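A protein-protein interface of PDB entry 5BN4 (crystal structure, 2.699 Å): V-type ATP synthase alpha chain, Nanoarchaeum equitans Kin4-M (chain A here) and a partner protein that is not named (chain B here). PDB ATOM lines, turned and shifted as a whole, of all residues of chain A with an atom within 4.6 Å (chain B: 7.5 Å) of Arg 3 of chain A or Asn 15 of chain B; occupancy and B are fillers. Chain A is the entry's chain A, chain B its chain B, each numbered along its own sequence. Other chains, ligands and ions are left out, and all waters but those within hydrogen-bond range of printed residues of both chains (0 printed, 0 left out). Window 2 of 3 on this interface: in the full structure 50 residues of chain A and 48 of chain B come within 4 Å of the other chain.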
ATOM      1  N   MET A   1      -6.912 -37.715 -11.697  1.00  0.00           N
ATOM      2  CA  MET A   1      -7.042 -36.397 -12.307  1.00  0.00           C
ATOM      3  C   MET A   1      -6.551 -35.302 -11.365  1.00  0.00           C
ATOM      4  O   MET A   1      -6.778 -34.115 -11.606  1.00  0.00           O
ATOM      5  CB  MET A   1      -8.486 -36.142 -12.719  1.00  0.00           C
ATOM      6  N   ASN A   2      -5.875 -35.708 -10.294  1.00  0.00           N
ATOM      7  CA  ASN A   2      -5.368 -34.768  -9.298  1.00  0.00           C
ATOM      8  C   ASN A   2      -4.191 -33.943  -9.808  1.00  0.00           C
ATOM      9  O   ASN A   2      -3.321 -34.452 -10.514  1.00  0.00           O
ATOM     10  CB  ASN A   2      -4.978 -35.498  -8.012  1.00  0.00           C
ATOM     11  CG  ASN A   2      -6.171 -36.105  -7.299  1.00  0.00           C
ATOM     12  OD1 ASN A   2      -7.276 -35.561  -7.336  1.00  0.00           O
ATOM     13  ND2 ASN A   2      -5.955 -37.238  -6.643  1.00  0.00           N
ATOM     14  N   ARG A   3      -4.166 -32.668  -9.435  1.00  0.00           N
ATOM     15  CA  ARG A   3      -3.142 -31.750  -9.913  1.00  0.00           C
ATOM     16  C   ARG A   3      -2.689 -30.785  -8.822  1.00  0.00           C
ATOM     17  O   ARG A   3      -3.512 -30.122  -8.192  1.00  0.00           O
ATOM     18  CB  ARG A   3      -3.673 -30.956 -11.109  1.00  0.00           C
ATOM     19  CG  ARG A   3      -2.780 -29.803 -11.540  1.00  0.00           C
ATOM     20  CD  ARG A   3      -3.554 -28.777 -12.356  1.00  0.00           C
ATOM     21  NE  ARG A   3      -2.723 -27.640 -12.744  1.00  0.00           N
ATOM     22  CZ  ARG A   3      -2.119 -27.523 -13.922  1.00  0.00           C
ATOM     23  NH1 ARG A   3      -2.254 -28.474 -14.835  1.00  0.00           N
ATOM     24  NH2 ARG A   3      -1.381 -26.453 -14.188  1.00  0.00           N
ATOM     25  N   ILE A   4      -1.380 -30.710  -8.604  1.00  0.00           N
ATOM     26  CA  ILE A   4      -0.810 -29.691  -7.732  1.00  0.00           C
ATOM     27  C   ILE A   4      -1.072 -28.323  -8.353  1.00  0.00           C
ATOM     28  O   ILE A   4      -0.831 -28.122  -9.540  1.00  0.00           O
ATOM     29  CB  ILE A   4       0.713 -29.878  -7.564  1.00  0.00           C
ATOM     30  CG1 ILE A   4       1.029 -31.243  -6.951  1.00  0.00           C
ATOM     31  CG2 ILE A   4       1.306 -28.756  -6.724  1.00  0.00           C
ATOM     32  CD1 ILE A   4       2.513 -31.529  -6.828  1.00  0.00           C
ATOM     33  N   ILE A   5      -1.583 -27.385  -7.564  1.00  0.00           N
ATOM     34  CA  ILE A   5      -1.843 -26.048  -8.087  1.00  0.00           C
ATOM     35  C   ILE A   5      -0.901 -25.015  -7.476  1.00  0.00           C
ATOM     36  O   ILE A   5      -0.799 -23.892  -7.969  1.00  0.00           O
ATOM     37  CB  ILE A   5      -3.308 -25.613  -7.876  1.00  0.00           C
ATOM     38  CG1 ILE A   5      -3.561 -25.253  -6.412  1.00  0.00           C
ATOM     39  CG2 ILE A   5      -4.264 -26.700  -8.353  1.00  0.00           C
ATOM     40  CD1 ILE A   5      -4.954 -24.723  -6.153  1.00  0.00           C
ATOM     41  N   ILE A  13      -0.853 -27.257  -2.341  1.00  0.00           N
ATOM     42  CA  ILE A  13      -2.281 -27.183  -2.613  1.00  0.00           C
ATOM     43  C   ILE A  13      -2.590 -27.909  -3.920  1.00  0.00           C
ATOM     44  O   ILE A  13      -1.942 -27.668  -4.939  1.00  0.00           O
ATOM     45  CB  ILE A  13      -2.759 -25.726  -2.702  1.00  0.00           C
ATOM     46  CG1 ILE A  13      -2.154 -24.902  -1.563  1.00  0.00           C
ATOM     47  CG2 ILE A  13      -4.277 -25.663  -2.669  1.00  0.00           C
ATOM     48  CD1 ILE A  13      -2.511 -23.433  -1.614  1.00  0.00           C
ATOM     49  N   ALA A  14      -3.576 -28.800  -3.885  1.00  0.00           N
ATOM     50  CA  ALA A  14      -3.894 -29.622  -5.049  1.00  0.00           C
ATOM     51  C   ALA A  14      -5.388 -29.674  -5.362  1.00  0.00           C
ATOM     52  O   ALA A  14      -6.228 -29.461  -4.488  1.00  0.00           O
ATOM     53  CB  ALA A  14      -3.341 -31.028  -4.872  1.00  0.00           C
ATOM     54  N   LYS A  15      -5.700 -29.970  -6.619  1.00  0.00           N
ATOM     55  CA  LYS A  15      -7.077 -30.071  -7.090  1.00  0.00           C
ATOM     56  C   LYS A  15      -7.512 -31.530  -7.184  1.00  0.00           C
ATOM     57  O   LYS A  15      -6.745 -32.383  -7.627  1.00  0.00           O
ATOM     58  CB  LYS A  15      -7.206 -29.406  -8.464  1.00  0.00           C
ATOM     59  CG  LYS A  15      -8.231 -30.058  -9.383  1.00  0.00           C
ATOM     60  CD  LYS A  15      -7.861 -29.877 -10.847  1.00  0.00           C
ATOM     61  CE  LYS A  15      -8.721 -30.754 -11.746  1.00  0.00           C
ATOM     62  NZ  LYS A  15      -8.304 -30.666 -13.173  1.00  0.00           N
ATOM     63  N   VAL A  56       4.307 -27.700 -11.148  1.00  0.00           N
ATOM     64  CA  VAL A  56       2.885 -27.484 -10.891  1.00  0.00           C
ATOM     65  C   VAL A  56       2.012 -28.642 -11.376  1.00  0.00           C
ATOM     66  O   VAL A  56       1.350 -29.297 -10.578  1.00  0.00           O
ATOM     67  CB  VAL A  56       2.385 -26.156 -11.502  1.00  0.00           C
ATOM     68  CG1 VAL A  56       0.865 -26.087 -11.467  1.00  0.00           C
ATOM     69  CG2 VAL A  56       2.982 -24.979 -10.756  1.00  0.00           C
ATOM     70  N   GLY A  57       2.030 -28.909 -12.679  1.00  0.00           N
ATOM     71  CA  GLY A  57       1.135 -29.890 -13.272  1.00  0.00           C
ATOM     72  C   GLY A  57       1.214 -31.318 -12.749  1.00  0.00           C
ATOM     73  O   GLY A  57       0.433 -32.173 -13.166  1.00  0.00           O
ATOM     74  N   GLU A  58       2.147 -31.577 -11.835  1.00  0.00           N
ATOM     75  CA  GLU A  58       2.365 -32.923 -11.306  1.00  0.00           C
ATOM     76  C   GLU A  58       1.135 -33.495 -10.595  1.00  0.00           C
ATOM     77  O   GLU A  58       0.334 -32.748 -10.034  1.00  0.00           O
ATOM     78  CB  GLU A  58       3.579 -32.939 -10.374  1.00  0.00           C
ATOM     79  CG  GLU A  58       4.878 -32.558 -11.059  1.00  0.00           C
ATOM     80  CD  GLU A  58       6.096 -32.894 -10.224  1.00  0.00           C
ATOM     81  OE1 GLU A  58       6.911 -31.984  -9.971  1.00  0.00           O
ATOM     82  OE2 GLU A  58       6.240 -34.072  -9.829  1.00  0.00           O
ATOM     83  N   GLU B  12       4.881 -14.613 -16.056  1.00  0.00           N
ATOM     84  CA  GLU B  12       4.013 -15.767 -16.268  1.00  0.00           C
ATOM     85  C   GLU B  12       4.799 -16.970 -16.780  1.00  0.00           C
ATOM     86  O   GLU B  12       5.633 -16.843 -17.678  1.00  0.00           O
ATOM     87  CB  GLU B  12       2.895 -15.429 -17.260  1.00  0.00           C
ATOM     88  CG  GLU B  12       1.533 -15.185 -16.627  1.00  0.00           C
ATOM     89  CD  GLU B  12       1.410 -13.809 -16.002  1.00  0.00           C
ATOM     90  OE1 GLU B  12       2.323 -12.980 -16.197  1.00  0.00           O
ATOM     91  OE2 GLU B  12       0.395 -13.557 -15.319  1.00  0.00           O
ATOM     92  N   LEU B  13       4.526 -18.136 -16.202  1.00  0.00           N
ATOM     93  CA  LEU B  13       5.122 -19.388 -16.656  1.00  0.00           C
ATOM     94  C   LEU B  13       4.051 -20.471 -16.735  1.00  0.00           C
ATOM     95  O   LEU B  13       3.085 -20.451 -15.972  1.00  0.00           O
ATOM     96  CB  LEU B  13       6.250 -19.824 -15.720  1.00  0.00           C
ATOM     97  CG  LEU B  13       7.499 -18.939 -15.689  1.00  0.00           C
ATOM     98  CD1 LEU B  13       8.522 -19.484 -14.702  1.00  0.00           C
ATOM     99  CD2 LEU B  13       8.105 -18.818 -17.077  1.00  0.00           C
ATOM    100  N   GLU B  14       4.226 -21.409 -17.663  1.00  0.00           N
ATOM    101  CA  GLU B  14       3.244 -22.467 -17.894  1.00  0.00           C
ATOM    102  C   GLU B  14       3.019 -23.306 -16.639  1.00  0.00           C
ATOM    103  O   GLU B  14       1.988 -23.191 -15.977  1.00  0.00           O
ATOM    104  CB  GLU B  14       3.674 -23.348 -19.057  1.00  0.00           C
ATOM    105  N   ASN B  15       3.990 -24.155 -16.321  1.00  0.00           N
ATOM    106  CA  ASN B  15       3.961 -24.918 -15.082  1.00  0.00           C
ATOM    107  C   ASN B  15       5.212 -24.649 -14.258  1.00  0.00           C
ATOM    108  O   ASN B  15       6.186 -25.399 -14.338  1.00  0.00           O
ATOM    109  CB  ASN B  15       3.804 -26.414 -15.363  1.00  0.00           C
ATOM    110  CG  ASN B  15       2.398 -26.780 -15.793  1.00  0.00           C
ATOM    111  OD1 ASN B  15       1.426 -26.148 -15.378  1.00  0.00           O
ATOM    112  ND2 ASN B  15       2.281 -27.807 -16.628  1.00  0.00           N
ATOM    113  N   PRO B  16       5.187 -23.561 -13.471  1.00  0.00           N
ATOM    114  CA  PRO B  16       6.320 -23.083 -12.669  1.00  0.00           C
ATOM    115  C   PRO B  16       6.884 -24.143 -11.726  1.00  0.00           C
ATOM    116  O   PRO B  16       6.128 -24.870 -11.082  1.00  0.00           O
ATOM    117  CB  PRO B  16       5.709 -21.937 -11.857  1.00  0.00           C
ATOM    118  CG  PRO B  16       4.579 -21.453 -12.690  1.00  0.00           C
ATOM    119  CD  PRO B  16       4.012 -22.680 -13.336  1.00  0.00           C
ATOM    120  N   MET B  17       8.208 -24.225 -11.659  1.00  0.00           N
ATOM    121  CA  MET B  17       8.873 -25.127 -10.730  1.00  0.00           C
ATOM    122  C   MET B  17       9.527 -24.313  -9.620  1.00  0.00           C
ATOM    123  O   MET B  17      10.189 -23.311  -9.888  1.00  0.00           O
ATOM    124  CB  MET B  17       9.929 -25.962 -11.455  1.00  0.00           C
ATOM    125  CG  MET B  17      10.657 -26.952 -10.560  1.00  0.00           C
ATOM    126  SD  MET B  17      12.151 -27.620 -11.316  1.00  0.00           S
ATOM    127  CE  MET B  17      11.493 -28.308 -12.832  1.00  0.00           C
ATOM    128  N   LEU B  18       9.336 -24.733  -8.375  1.00  0.00           N
ATOM    129  CA  LEU B  18       9.944 -24.030  -7.252  1.00  0.00           C
ATOM    130  C   LEU B  18      11.454 -24.239  -7.249  1.00  0.00           C
ATOM    131  O   LEU B  18      11.933 -25.372  -7.171  1.00  0.00           O
ATOM    132  CB  LEU B  18       9.343 -24.493  -5.922  1.00  0.00           C
ATOM    133  CG  LEU B  18       8.763 -23.398  -5.020  1.00  0.00           C
ATOM    134  CD1 LEU B  18       8.556 -23.919  -3.605  1.00  0.00           C
ATOM    135  CD2 LEU B  18       9.642 -22.153  -5.015  1.00  0.00           C
ATOM    136  N   GLU B  20      13.379 -23.250  -9.738  1.00  0.00           N
ATOM    137  CA  GLU B  20      13.797 -23.395 -11.129  1.00  0.00           C
ATOM    138  C   GLU B  20      14.676 -22.238 -11.589  1.00  0.00           C
ATOM    139  O   GLU B  20      14.407 -21.077 -11.274  1.00  0.00           O
ATOM    140  CB  GLU B  20      12.573 -23.501 -12.042  1.00  0.00           C
ATOM    141  CG  GLU B  20      12.902 -23.709 -13.511  1.00  0.00           C
ATOM    142  CD  GLU B  20      11.664 -23.737 -14.384  1.00  0.00           C
ATOM    143  OE1 GLU B  20      11.773 -24.145 -15.560  1.00  0.00           O
ATOM    144  OE2 GLU B  20      10.582 -23.348 -13.895  1.00  0.00           O
ATOM    145  N   ALA B  34       5.758 -19.934  -6.636  1.00  0.00           N
ATOM    146  CA  ALA B  34       5.003 -20.540  -7.728  1.00  0.00           C
ATOM    147  C   ALA B  34       3.523 -20.697  -7.393  1.00  0.00           C
ATOM    148  O   ALA B  34       3.129 -21.640  -6.703  1.00  0.00           O
ATOM    149  CB  ALA B  34       5.607 -21.888  -8.104  1.00  0.00           C
ATOM    150  N   TYR B  35       2.710 -19.769  -7.886  1.00  0.00           N
ATOM    151  CA  TYR B  35       1.268 -19.859  -7.740  1.00  0.00           C
ATOM    152  C   TYR B  35       0.693 -20.798  -8.783  1.00  0.00           C
ATOM    153  O   TYR B  35       1.042 -21.978  -8.824  1.00  0.00           O
ATOM    154  N   GLU B  36      -0.185 -20.277  -9.632  1.00  0.00           N
ATOM    155  CA  GLU B  36      -0.738 -21.066 -10.727  1.00  0.00           C
ATOM    156  C   GLU B  36       0.099 -20.871 -11.986  1.00  0.00           C
ATOM    157  O   GLU B  36       0.898 -21.735 -12.354  1.00  0.00           O
ATOM    158  CB  GLU B  36      -2.186 -20.684 -10.982  1.00  0.00           C
ATOM    159  N   ASN B  37      -0.087 -19.730 -12.641  1.00  0.00           N
ATOM    160  CA  ASN B  37       0.694 -19.387 -13.814  1.00  0.00           C
ATOM    161  C   ASN B  37       1.693 -18.292 -13.499  1.00  0.00           C
ATOM    162  O   ASN B  37       2.551 -17.967 -14.319  1.00  0.00           O
ATOM    163  N   ARG B  56      14.003 -21.499 -19.824  1.00  0.00           N
ATOM    164  CA  ARG B  56      13.855 -22.233 -18.572  1.00  0.00           C
ATOM    165  C   ARG B  56      14.710 -23.494 -18.533  1.00  0.00           C
ATOM    166  O   ARG B  56      14.480 -24.432 -19.296  1.00  0.00           O
ATOM    167  CB  ARG B  56      12.388 -22.604 -18.345  1.00  0.00           C
ATOM    168  CG  ARG B  56      11.446 -21.415 -18.266  1.00  0.00           C
ATOM    169  CD  ARG B  56       9.992 -21.861 -18.198  1.00  0.00           C
ATOM    170  NE  ARG B  56       9.715 -22.665 -17.010  1.00  0.00           N
ATOM    171  CZ  ARG B  56       8.515 -23.146 -16.698  1.00  0.00           C
ATOM    172  NH1 ARG B  56       7.476 -22.905 -17.486  1.00  0.00           N
ATOM    173  NH2 ARG B  56       8.353 -23.867 -15.597  1.00  0.00           N
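The guanidinium group of Arg 3 of chain A is in hydrogen-bond range of the side-chain amide oxygen of Asn 15 of chain B, 3.1 Å away. O of Pro 16 of chain B sits close to N of Val 56 of chain A (3.4 Å). The backbone carbonyl oxygen of Ile 5 of chain A sits close to the backbone carbonyl oxygen of Tyr 35 of chain B.
N of Lys 15 of chain A lies within hydrogen-bond range of O of Arg 3 of chain A, 2.7 Å away. The backbone carbonyl oxygen (O) of Ile 4 of chain A lies close to the backbone carbonyl oxygen (O) of Val 56 of chain A, at 2.7 Å. O of Ile 13 of chain A is in hydrogen-bond range of N of Ile 5 of chain A, at 2.7 Å. O of Asn 15 of chain B sits at hydrogen-bond distance from NH2 of Arg 56 of chain B.
Among the printed residues, pairs that only touch across the chains: Gly 57 of chain A with Asn 15 of chain B, Ile 5 of chain A with Glu 36 of chain B and Val 56 of chain A with Asn 15 of chain B.
Of chain B, only Asn 15 comes within 4 Å of Arg 3 of chain A. Asn 15 of chain B touches just these residues of chain A: Arg 3, Val 56 and Gly 57. Of the printed residues of chain B, Gly 57 of chain A touches Asn 15. Printed residues of chain B within 4 Å of Ile 5 of chain A: Tyr 35 and Glu 36. Of the printed residues of chain A, Tyr 35 of chain B touches Ile 5. Of the printed residues of chain A, Glu 36 of chain B touches Ile 5. Printed residues of chain B within 4 Å of Val 56 of chain A: Asn 15 (3.95 Å) and Pro 16 (3.2 Å). Leu 18 of chain B touches none of the printed residues of chain A. Glu 14 of chain B touches none of the printed residues of chain A. The nearest printed residue of chain A that does not touch Asn 15 of chain B is Glu 58 of chain A (6.1 Å).
Of the 13 printed residues of chain B, 4 touch a printed residue of chain A. Hydrophobic or aromatic side chains of chain B that line the printed part of chain A: Pro 16. Of the 11 printed residues of chain A, 4 touch a printed residue of chain B. Printed residues of chain A that touch a printed residue of chain B: Arg 3, Ile 5, Val 56 and Gly 57. Hydrophobic or aromatic side chains of chain A within 4 Å of the printed part of chain B: Val 56.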
